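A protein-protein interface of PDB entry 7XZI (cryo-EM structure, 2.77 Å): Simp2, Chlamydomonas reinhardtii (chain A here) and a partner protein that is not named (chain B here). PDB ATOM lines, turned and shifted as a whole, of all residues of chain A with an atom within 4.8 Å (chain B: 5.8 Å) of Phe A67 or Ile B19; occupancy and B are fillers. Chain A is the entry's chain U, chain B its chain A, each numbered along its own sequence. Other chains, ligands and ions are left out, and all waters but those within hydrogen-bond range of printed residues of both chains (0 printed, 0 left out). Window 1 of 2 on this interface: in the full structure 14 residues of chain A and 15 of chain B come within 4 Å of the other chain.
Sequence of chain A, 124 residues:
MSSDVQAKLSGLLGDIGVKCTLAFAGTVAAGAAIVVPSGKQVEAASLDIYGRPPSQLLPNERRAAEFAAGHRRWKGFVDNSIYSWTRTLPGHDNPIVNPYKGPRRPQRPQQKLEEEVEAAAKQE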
ATOM      1  N   ARG A  63       6.546   0.809 -20.784  1.00  0.00           N
ATOM      2  CA  ARG A  63       5.518  -0.185 -20.499  1.00  0.00           C
ATOM      3  C   ARG A  63       4.658  -0.454 -21.726  1.00  0.00           C
ATOM      4  O   ARG A  63       4.292  -1.604 -21.991  1.00  0.00           O
ATOM      5  CB  ARG A  63       4.651   0.274 -19.327  1.00  0.00           C
ATOM      6  CG  ARG A  63       5.403   0.429 -18.014  1.00  0.00           C
ATOM      7  CD  ARG A  63       4.486   0.884 -16.883  1.00  0.00           C
ATOM      8  NE  ARG A  63       3.431  -0.079 -16.598  1.00  0.00           N
ATOM      9  CZ  ARG A  63       2.173   0.041 -17.009  1.00  0.00           C
ATOM     10  NH1 ARG A  63       1.776   1.081 -17.724  1.00  0.00           N
ATOM     11  NH2 ARG A  63       1.294  -0.904 -16.692  1.00  0.00           N
ATOM     12  N   ALA A  64       4.320   0.593 -22.481  1.00  0.00           N
ATOM     13  CA  ALA A  64       3.539   0.405 -23.699  1.00  0.00           C
ATOM     14  C   ALA A  64       4.301  -0.427 -24.722  1.00  0.00           C
ATOM     15  O   ALA A  64       3.725  -1.307 -25.371  1.00  0.00           O
ATOM     16  CB  ALA A  64       3.150   1.760 -24.290  1.00  0.00           C
ATOM     17  N   ALA A  65       5.600  -0.162 -24.881  1.00  0.00           N
ATOM     18  CA  ALA A  65       6.404  -0.947 -25.816  1.00  0.00           C
ATOM     19  C   ALA A  65       6.479  -2.409 -25.386  1.00  0.00           C
ATOM     20  O   ALA A  65       6.364  -3.322 -26.214  1.00  0.00           O
ATOM     21  CB  ALA A  65       7.805  -0.345 -25.934  1.00  0.00           C
ATOM     22  N   GLU A  66       6.678  -2.647 -24.087  1.00  0.00           N
ATOM     23  CA  GLU A  66       6.725  -4.018 -23.587  1.00  0.00           C
ATOM     24  C   GLU A  66       5.391  -4.726 -23.788  1.00  0.00           C
ATOM     25  O   GLU A  66       5.354  -5.907 -24.152  1.00  0.00           O
ATOM     26  CB  GLU A  66       7.120  -4.026 -22.111  1.00  0.00           C
ATOM     27  CG  GLU A  66       8.530  -3.530 -21.852  1.00  0.00           C
ATOM     28  CD  GLU A  66       8.877  -3.512 -20.378  1.00  0.00           C
ATOM     29  OE1 GLU A  66       8.016  -3.894 -19.558  1.00  0.00           O
ATOM     30  OE2 GLU A  66      10.011  -3.114 -20.040  1.00  0.00           O
ATOM     31  N   PHE A  67       4.283  -4.018 -23.555  1.00  0.00           N
ATOM     32  CA  PHE A  67       2.967  -4.599 -23.790  1.00  0.00           C
ATOM     33  C   PHE A  67       2.770  -4.938 -25.261  1.00  0.00           C
ATOM     34  O   PHE A  67       2.195  -5.979 -25.590  1.00  0.00           O
ATOM     35  CB  PHE A  67       1.876  -3.641 -23.313  1.00  0.00           C
ATOM     36  CG  PHE A  67       0.486  -4.079 -23.675  1.00  0.00           C
ATOM     37  CD1 PHE A  67      -0.220  -4.934 -22.849  1.00  0.00           C
ATOM     38  CD2 PHE A  67      -0.114  -3.638 -24.843  1.00  0.00           C
ATOM     39  CE1 PHE A  67      -1.498  -5.338 -23.180  1.00  0.00           C
ATOM     40  CE2 PHE A  67      -1.388  -4.039 -25.179  1.00  0.00           C
ATOM     41  CZ  PHE A  67      -2.082  -4.891 -24.347  1.00  0.00           C
ATOM     42  N   ALA A  68       3.216  -4.058 -26.158  1.00  0.00           N
ATOM     43  CA  ALA A  68       3.098  -4.337 -27.585  1.00  0.00           C
ATOM     44  C   ALA A  68       3.893  -5.578 -27.970  1.00  0.00           C
ATOM     45  O   ALA A  68       3.398  -6.437 -28.714  1.00  0.00           O
ATOM     46  CB  ALA A  68       3.560  -3.128 -28.398  1.00  0.00           C
ATOM     47  N   ALA A  69       5.124  -5.693 -27.466  1.00  0.00           N
ATOM     48  CA  ALA A  69       5.931  -6.875 -27.757  1.00  0.00           C
ATOM     49  C   ALA A  69       5.272  -8.141 -27.218  1.00  0.00           C
ATOM     50  O   ALA A  69       5.221  -9.168 -27.907  1.00  0.00           O
ATOM     51  CB  ALA A  69       7.336  -6.709 -27.178  1.00  0.00           C
ATOM     52  N   GLY A  70       4.758  -8.082 -25.988  1.00  0.00           N
ATOM     53  CA  GLY A  70       4.093  -9.242 -25.417  1.00  0.00           C
ATOM     54  C   GLY A  70       2.845  -9.640 -26.182  1.00  0.00           C
ATOM     55  O   GLY A  70       2.577 -10.828 -26.373  1.00  0.00           O
ATOM     56  N   HIS A  71       2.059  -8.654 -26.618  1.00  0.00           N
ATOM     57  CA  HIS A  71       0.859  -8.951 -27.391  1.00  0.00           C
ATOM     58  C   HIS A  71       1.211  -9.570 -28.739  1.00  0.00           C
ATOM     59  O   HIS A  71       0.538 -10.503 -29.198  1.00  0.00           O
ATOM     60  CB  HIS A  71       0.028  -7.683 -27.580  1.00  0.00           C
ATOM     61  CG  HIS A  71      -1.354  -7.938 -28.092  1.00  0.00           C
ATOM     62  ND1 HIS A  71      -2.156  -8.945 -27.598  1.00  0.00           N
ATOM     63  CD2 HIS A  71      -2.079  -7.316 -29.052  1.00  0.00           C
ATOM     64  CE1 HIS A  71      -3.314  -8.933 -28.233  1.00  0.00           C
ATOM     65  NE2 HIS A  71      -3.293  -7.955 -29.119  1.00  0.00           N
ATOM     66  N   LYS B  14      -6.497   2.419 -15.630  1.00  0.00           N
ATOM     67  CA  LYS B  14      -6.261   3.629 -16.410  1.00  0.00           C
ATOM     68  C   LYS B  14      -5.025   3.490 -17.289  1.00  0.00           C
ATOM     69  O   LYS B  14      -5.020   3.936 -18.443  1.00  0.00           O
ATOM     70  CB  LYS B  14      -6.124   4.836 -15.484  1.00  0.00           C
ATOM     71  CG  LYS B  14      -7.411   5.227 -14.787  1.00  0.00           C
ATOM     72  CD  LYS B  14      -7.182   6.398 -13.851  1.00  0.00           C
ATOM     73  CE  LYS B  14      -8.459   6.783 -13.129  1.00  0.00           C
ATOM     74  NZ  LYS B  14      -8.235   7.914 -12.190  1.00  0.00           N
ATOM     75  N   ASP B  15      -3.963   2.883 -16.758  1.00  0.00           N
ATOM     76  CA  ASP B  15      -2.767   2.656 -17.562  1.00  0.00           C
ATOM     77  C   ASP B  15      -3.062   1.731 -18.737  1.00  0.00           C
ATOM     78  O   ASP B  15      -2.591   1.966 -19.856  1.00  0.00           O
ATOM     79  CB  ASP B  15      -1.647   2.085 -16.693  1.00  0.00           C
ATOM     80  CG  ASP B  15      -1.194   3.051 -15.616  1.00  0.00           C
ATOM     81  OD1 ASP B  15      -1.791   4.142 -15.506  1.00  0.00           O
ATOM     82  OD2 ASP B  15      -0.240   2.723 -14.880  1.00  0.00           O
ATOM     83  N   TYR B  16      -3.846   0.677 -18.502  1.00  0.00           N
ATOM     84  CA  TYR B  16      -4.219  -0.225 -19.588  1.00  0.00           C
ATOM     85  C   TYR B  16      -5.051   0.494 -20.642  1.00  0.00           C
ATOM     86  O   TYR B  16      -4.871   0.270 -21.844  1.00  0.00           O
ATOM     87  CB  TYR B  16      -4.977  -1.432 -19.035  1.00  0.00           C
ATOM     88  CG  TYR B  16      -5.621  -2.291 -20.099  1.00  0.00           C
ATOM     89  CD1 TYR B  16      -4.863  -3.155 -20.877  1.00  0.00           C
ATOM     90  CD2 TYR B  16      -6.990  -2.241 -20.321  1.00  0.00           C
ATOM     91  CE1 TYR B  16      -5.450  -3.942 -21.849  1.00  0.00           C
ATOM     92  CE2 TYR B  16      -7.585  -3.022 -21.289  1.00  0.00           C
ATOM     93  CZ  TYR B  16      -6.812  -3.871 -22.050  1.00  0.00           C
ATOM     94  OH  TYR B  16      -7.405  -4.650 -23.014  1.00  0.00           O
ATOM     95  N   VAL B  17      -5.977   1.351 -20.210  1.00  0.00           N
ATOM     96  CA  VAL B  17      -6.793   2.106 -21.158  1.00  0.00           C
ATOM     97  C   VAL B  17      -5.921   3.048 -21.981  1.00  0.00           C
ATOM     98  O   VAL B  17      -6.112   3.194 -23.194  1.00  0.00           O
ATOM     99  CB  VAL B  17      -7.911   2.862 -20.418  1.00  0.00           C
ATOM    100  CG1 VAL B  17      -8.636   3.800 -21.364  1.00  0.00           C
ATOM    101  CG2 VAL B  17      -8.891   1.878 -19.802  1.00  0.00           C
ATOM    102  N   GLU B  18      -4.953   3.702 -21.335  1.00  0.00           N
ATOM    103  CA  GLU B  18      -4.028   4.568 -22.061  1.00  0.00           C
ATOM    104  C   GLU B  18      -3.217   3.778 -23.080  1.00  0.00           C
ATOM    105  O   GLU B  18      -3.016   4.230 -24.214  1.00  0.00           O
ATOM    106  CB  GLU B  18      -3.099   5.282 -21.081  1.00  0.00           C
ATOM    107  CG  GLU B  18      -2.055   6.167 -21.745  1.00  0.00           C
ATOM    108  CD  GLU B  18      -0.831   6.375 -20.872  1.00  0.00           C
ATOM    109  OE1 GLU B  18      -0.658   5.610 -19.901  1.00  0.00           O
ATOM    110  OE2 GLU B  18      -0.044   7.302 -21.157  1.00  0.00           O
ATOM    111  N   ILE B  19      -2.738   2.595 -22.690  1.00  0.00           N
ATOM    112  CA  ILE B  19      -1.969   1.760 -23.608  1.00  0.00           C
ATOM    113  C   ILE B  19      -2.828   1.335 -24.794  1.00  0.00           C
ATOM    114  O   ILE B  19      -2.371   1.345 -25.942  1.00  0.00           O
ATOM    115  CB  ILE B  19      -1.383   0.547 -22.862  1.00  0.00           C
ATOM    116  CG1 ILE B  19      -0.326   0.993 -21.849  1.00  0.00           C
ATOM    117  CG2 ILE B  19      -0.780  -0.434 -23.839  1.00  0.00           C
ATOM    118  CD1 ILE B  19       0.307  -0.152 -21.082  1.00  0.00           C
ATOM    119  N   THR B  20      -4.083   0.955 -24.537  1.00  0.00           N
ATOM    120  CA  THR B  20      -4.980   0.582 -25.627  1.00  0.00           C
ATOM    121  C   THR B  20      -5.238   1.759 -26.559  1.00  0.00           C
ATOM    122  O   THR B  20      -5.303   1.590 -27.782  1.00  0.00           O
ATOM    123  CB  THR B  20      -6.302   0.047 -25.074  1.00  0.00           C
ATOM    124  OG1 THR B  20      -6.874   1.008 -24.178  1.00  0.00           O
ATOM    125  CG2 THR B  20      -6.085  -1.269 -24.342  1.00  0.00           C
ATOM    126  N   HIS B  21      -5.401   2.960 -25.998  1.00  0.00           N
ATOM    127  CA  HIS B  21      -5.591   4.145 -26.829  1.00  0.00           C
ATOM    128  C   HIS B  21      -4.357   4.433 -27.673  1.00  0.00           C
ATOM    129  O   HIS B  21      -4.470   4.889 -28.817  1.00  0.00           O
ATOM    130  CB  HIS B  21      -5.936   5.352 -25.957  1.00  0.00           C
ATOM    131  CG  HIS B  21      -7.327   5.323 -25.409  1.00  0.00           C
ATOM    132  ND1 HIS B  21      -7.799   6.268 -24.524  1.00  0.00           N
ATOM    133  CD2 HIS B  21      -8.352   4.465 -25.622  1.00  0.00           C
ATOM    134  CE1 HIS B  21      -9.051   5.992 -24.214  1.00  0.00           C
ATOM    135  NE2 HIS B  21      -9.412   4.903 -24.868  1.00  0.00           N
ATOM    136  N   LYS B  22      -3.168   4.184 -27.121  1.00  0.00           N
ATOM    137  CA  LYS B  22      -1.935   4.439 -27.861  1.00  0.00           C
ATOM    138  C   LYS B  22      -1.814   3.529 -29.079  1.00  0.00           C
ATOM    139  O   LYS B  22      -1.222   3.916 -30.094  1.00  0.00           O
ATOM    140  CB  LYS B  22      -0.730   4.267 -26.934  1.00  0.00           C
ATOM    141  CG  LYS B  22       0.624   4.398 -27.614  1.00  0.00           C
ATOM    142  CD  LYS B  22       0.776   5.742 -28.308  1.00  0.00           C
ATOM    143  CE  LYS B  22       2.085   5.819 -29.077  1.00  0.00           C
ATOM    144  NZ  LYS B  22       2.234   7.117 -29.794  1.00  0.00           N
ATOM    145  N   LEU B  23      -2.389   2.331 -29.011  1.00  0.00           N
ATOM    146  CA  LEU B  23      -2.203   1.336 -30.060  1.00  0.00           C
ATOM    147  C   LEU B  23      -3.151   1.510 -31.239  1.00  0.00           C
ATOM    148  O   LEU B  23      -3.129   0.677 -32.151  1.00  0.00           O
ATOM    149  CB  LEU B  23      -2.355  -0.074 -29.481  1.00  0.00           C
ATOM    150  CG  LEU B  23      -1.222  -0.527 -28.560  1.00  0.00           C
ATOM    151  CD1 LEU B  23      -1.406  -1.976 -28.141  1.00  0.00           C
ATOM    152  CD2 LEU B  23       0.123  -0.329 -29.242  1.00  0.00           C
ATOM    153  N   ILE B  24      -3.982   2.553 -31.248  1.00  0.00           N
ATOM    154  CA  ILE B  24      -4.834   2.808 -32.407  1.00  0.00           C
ATOM    155  C   ILE B  24      -3.983   3.074 -33.642  1.00  0.00           C
ATOM    156  O   ILE B  24      -4.289   2.597 -34.742  1.00  0.00           O
ATOM    157  CB  ILE B  24      -5.794   3.979 -32.120  1.00  0.00           C
ATOM    158  CG1 ILE B  24      -6.691   3.657 -30.926  1.00  0.00           C
ATOM    159  CG2 ILE B  24      -6.639   4.292 -33.345  1.00  0.00           C
ATOM    160  CD1 ILE B  24      -7.627   4.783 -30.554  1.00  0.00           C
ATOM    161  N   LEU B  29      -7.148  -2.576 -31.772  1.00  0.00           N
ATOM    162  CA  LEU B  29      -7.782  -3.707 -31.115  1.00  0.00           C
ATOM    163  C   LEU B  29      -9.279  -3.683 -31.391  1.00  0.00           C
ATOM    164  O   LEU B  29      -9.863  -2.623 -31.631  1.00  0.00           O
ATOM    165  CB  LEU B  29      -7.531  -3.688 -29.601  1.00  0.00           C
ATOM    166  CG  LEU B  29      -6.173  -4.138 -29.047  1.00  0.00           C
ATOM    167  CD1 LEU B  29      -5.050  -3.179 -29.418  1.00  0.00           C
ATOM    168  CD2 LEU B  29      -6.249  -4.310 -27.536  1.00  0.00           C
ATOM    169  N   ALA B  37      -5.255  -9.378 -24.849  1.00  0.00           N
ATOM    170  CA  ALA B  37      -4.676  -8.157 -24.300  1.00  0.00           C
ATOM    171  C   ALA B  37      -4.846  -8.097 -22.788  1.00  0.00           C
ATOM    172  O   ALA B  37      -3.904  -7.763 -22.059  1.00  0.00           O
ATOM    173  CB  ALA B  37      -5.307  -6.932 -24.963  1.00  0.00           C
ATOM    174  N   VAL B  38      -6.044  -8.418 -22.299  1.00  0.00           N
ATOM    175  CA  VAL B  38      -6.281  -8.422 -20.860  1.00  0.00           C
ATOM    176  C   VAL B  38      -5.378  -9.439 -20.176  1.00  0.00           C
ATOM    177  O   VAL B  38      -4.791  -9.161 -19.125  1.00  0.00           O
ATOM    178  CB  VAL B  38      -7.769  -8.690 -20.564  1.00  0.00           C
ATOM    179  CG1 VAL B  38      -7.987  -8.882 -19.074  1.00  0.00           C
ATOM    180  CG2 VAL B  38      -8.622  -7.549 -21.084  1.00  0.00           C
ATOM    181  N   THR B  40      -2.419 -10.711 -21.192  1.00  0.00           N
ATOM    182  CA  THR B  40      -1.011 -10.333 -21.187  1.00  0.00           C
ATOM    183  C   THR B  40      -0.758  -9.143 -20.267  1.00  0.00           C
ATOM    184  O   THR B  40       0.269  -9.097 -19.582  1.00  0.00           O
ATOM    185  CB  THR B  40      -0.518 -10.052 -22.612  1.00  0.00           C
ATOM    186  OG1 THR B  40       0.893  -9.799 -22.588  1.00  0.00           O
ATOM    187  CG2 THR B  40      -1.225  -8.861 -23.228  1.00  0.00           C
ATOM    188  N   TYR B  41      -1.690  -8.184 -20.207  1.00  0.00           N
ATOM    189  CA  TYR B  41      -1.508  -7.060 -19.297  1.00  0.00           C
ATOM    190  C   TYR B  41      -1.592  -7.509 -17.844  1.00  0.00           C
ATOM    191  O   TYR B  41      -0.858  -7.000 -16.991  1.00  0.00           O
ATOM    192  CB  TYR B  41      -2.536  -5.966 -19.581  1.00  0.00           C
ATOM    193  CG  TYR B  41      -2.309  -4.708 -18.769  1.00  0.00           C
ATOM    194  CD1 TYR B  41      -1.353  -3.777 -19.150  1.00  0.00           C
ATOM    195  CD2 TYR B  41      -3.046  -4.456 -17.619  1.00  0.00           C
ATOM    196  CE1 TYR B  41      -1.140  -2.629 -18.411  1.00  0.00           C
ATOM    197  CE2 TYR B  41      -2.839  -3.311 -16.874  1.00  0.00           C
ATOM    198  CZ  TYR B  41      -1.885  -2.401 -17.276  1.00  0.00           C
ATOM    199  OH  TYR B  41      -1.674  -1.259 -16.539  1.00  0.00           O
ATOM    200  N   PHE B  44       1.711  -9.117 -17.074  1.00  0.00           N
ATOM    201  CA  PHE B  44       2.723  -8.078 -16.909  1.00  0.00           C
ATOM    202  C   PHE B  44       2.591  -7.392 -15.555  1.00  0.00           C
ATOM    203  O   PHE B  44       3.590  -7.159 -14.864  1.00  0.00           O
ATOM    204  CB  PHE B  44       2.615  -7.048 -18.033  1.00  0.00           C
ATOM    205  CG  PHE B  44       3.447  -7.370 -19.239  1.00  0.00           C
ATOM    206  CD1 PHE B  44       4.827  -7.292 -19.182  1.00  0.00           C
ATOM    207  CD2 PHE B  44       2.849  -7.732 -20.433  1.00  0.00           C
ATOM    208  CE1 PHE B  44       5.594  -7.582 -20.291  1.00  0.00           C
ATOM    209  CE2 PHE B  44       3.610  -8.023 -21.545  1.00  0.00           C
ATOM    210  CZ  PHE B  44       4.985  -7.948 -21.474  1.00  0.00           C
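Of the printed residues of chain B, Glu A66 touches Phe B44 (3.4 Å). Of chain B, only Ile B19, Leu B23, Ala B37, Thr B40 and Tyr B41 come within 4 Å of Phe A67. Of the printed residues of chain B, His A71 touches Ala B37. Lys B14 touches none of the printed residues of chain A. Of the printed residues of chain A, Asp B15 touches Arg A63. Ile B19 touches just these residues of chain A: Arg A63 and Phe A67. Of the printed residues of chain A, Tyr B41 touches Arg A63 (3.0 Å) and Phe A67 (3.8 Å). The nearest printed residue of chain A that does not touch Phe B44 is Gly A70 (4.1 Å).
Printed residues of chain B that touch a printed residue of chain A: Asp B15, Ile B19, Leu B23, Ala B37, Thr B40, Tyr B41 and Phe B44. Among the printed residues, Asp or Glu carboxylates within 4 Å of a Lys or Arg side-chain nitrogen of the other chain: Arg A63 with Asp B15.
Among the printed residues, pairs that only touch across the chains: Glu A66 with Phe B44, Phe A67 with Ile B19, Phe A67 with Thr B40, Phe A67 with Ala B37, Phe A67 with Leu B23, Phe A67 with Tyr B41, Arg A63 with Ile B19 and His A71 with Ala B37.
NH2 of Arg A63 is in hydrogen-bond range of OH of Tyr B41 (3.0 Å). The side-chain carboxylate (OD2) of Asp B15 lies within salt-bridge range of the guanidinium group (NH1) of Arg A63.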
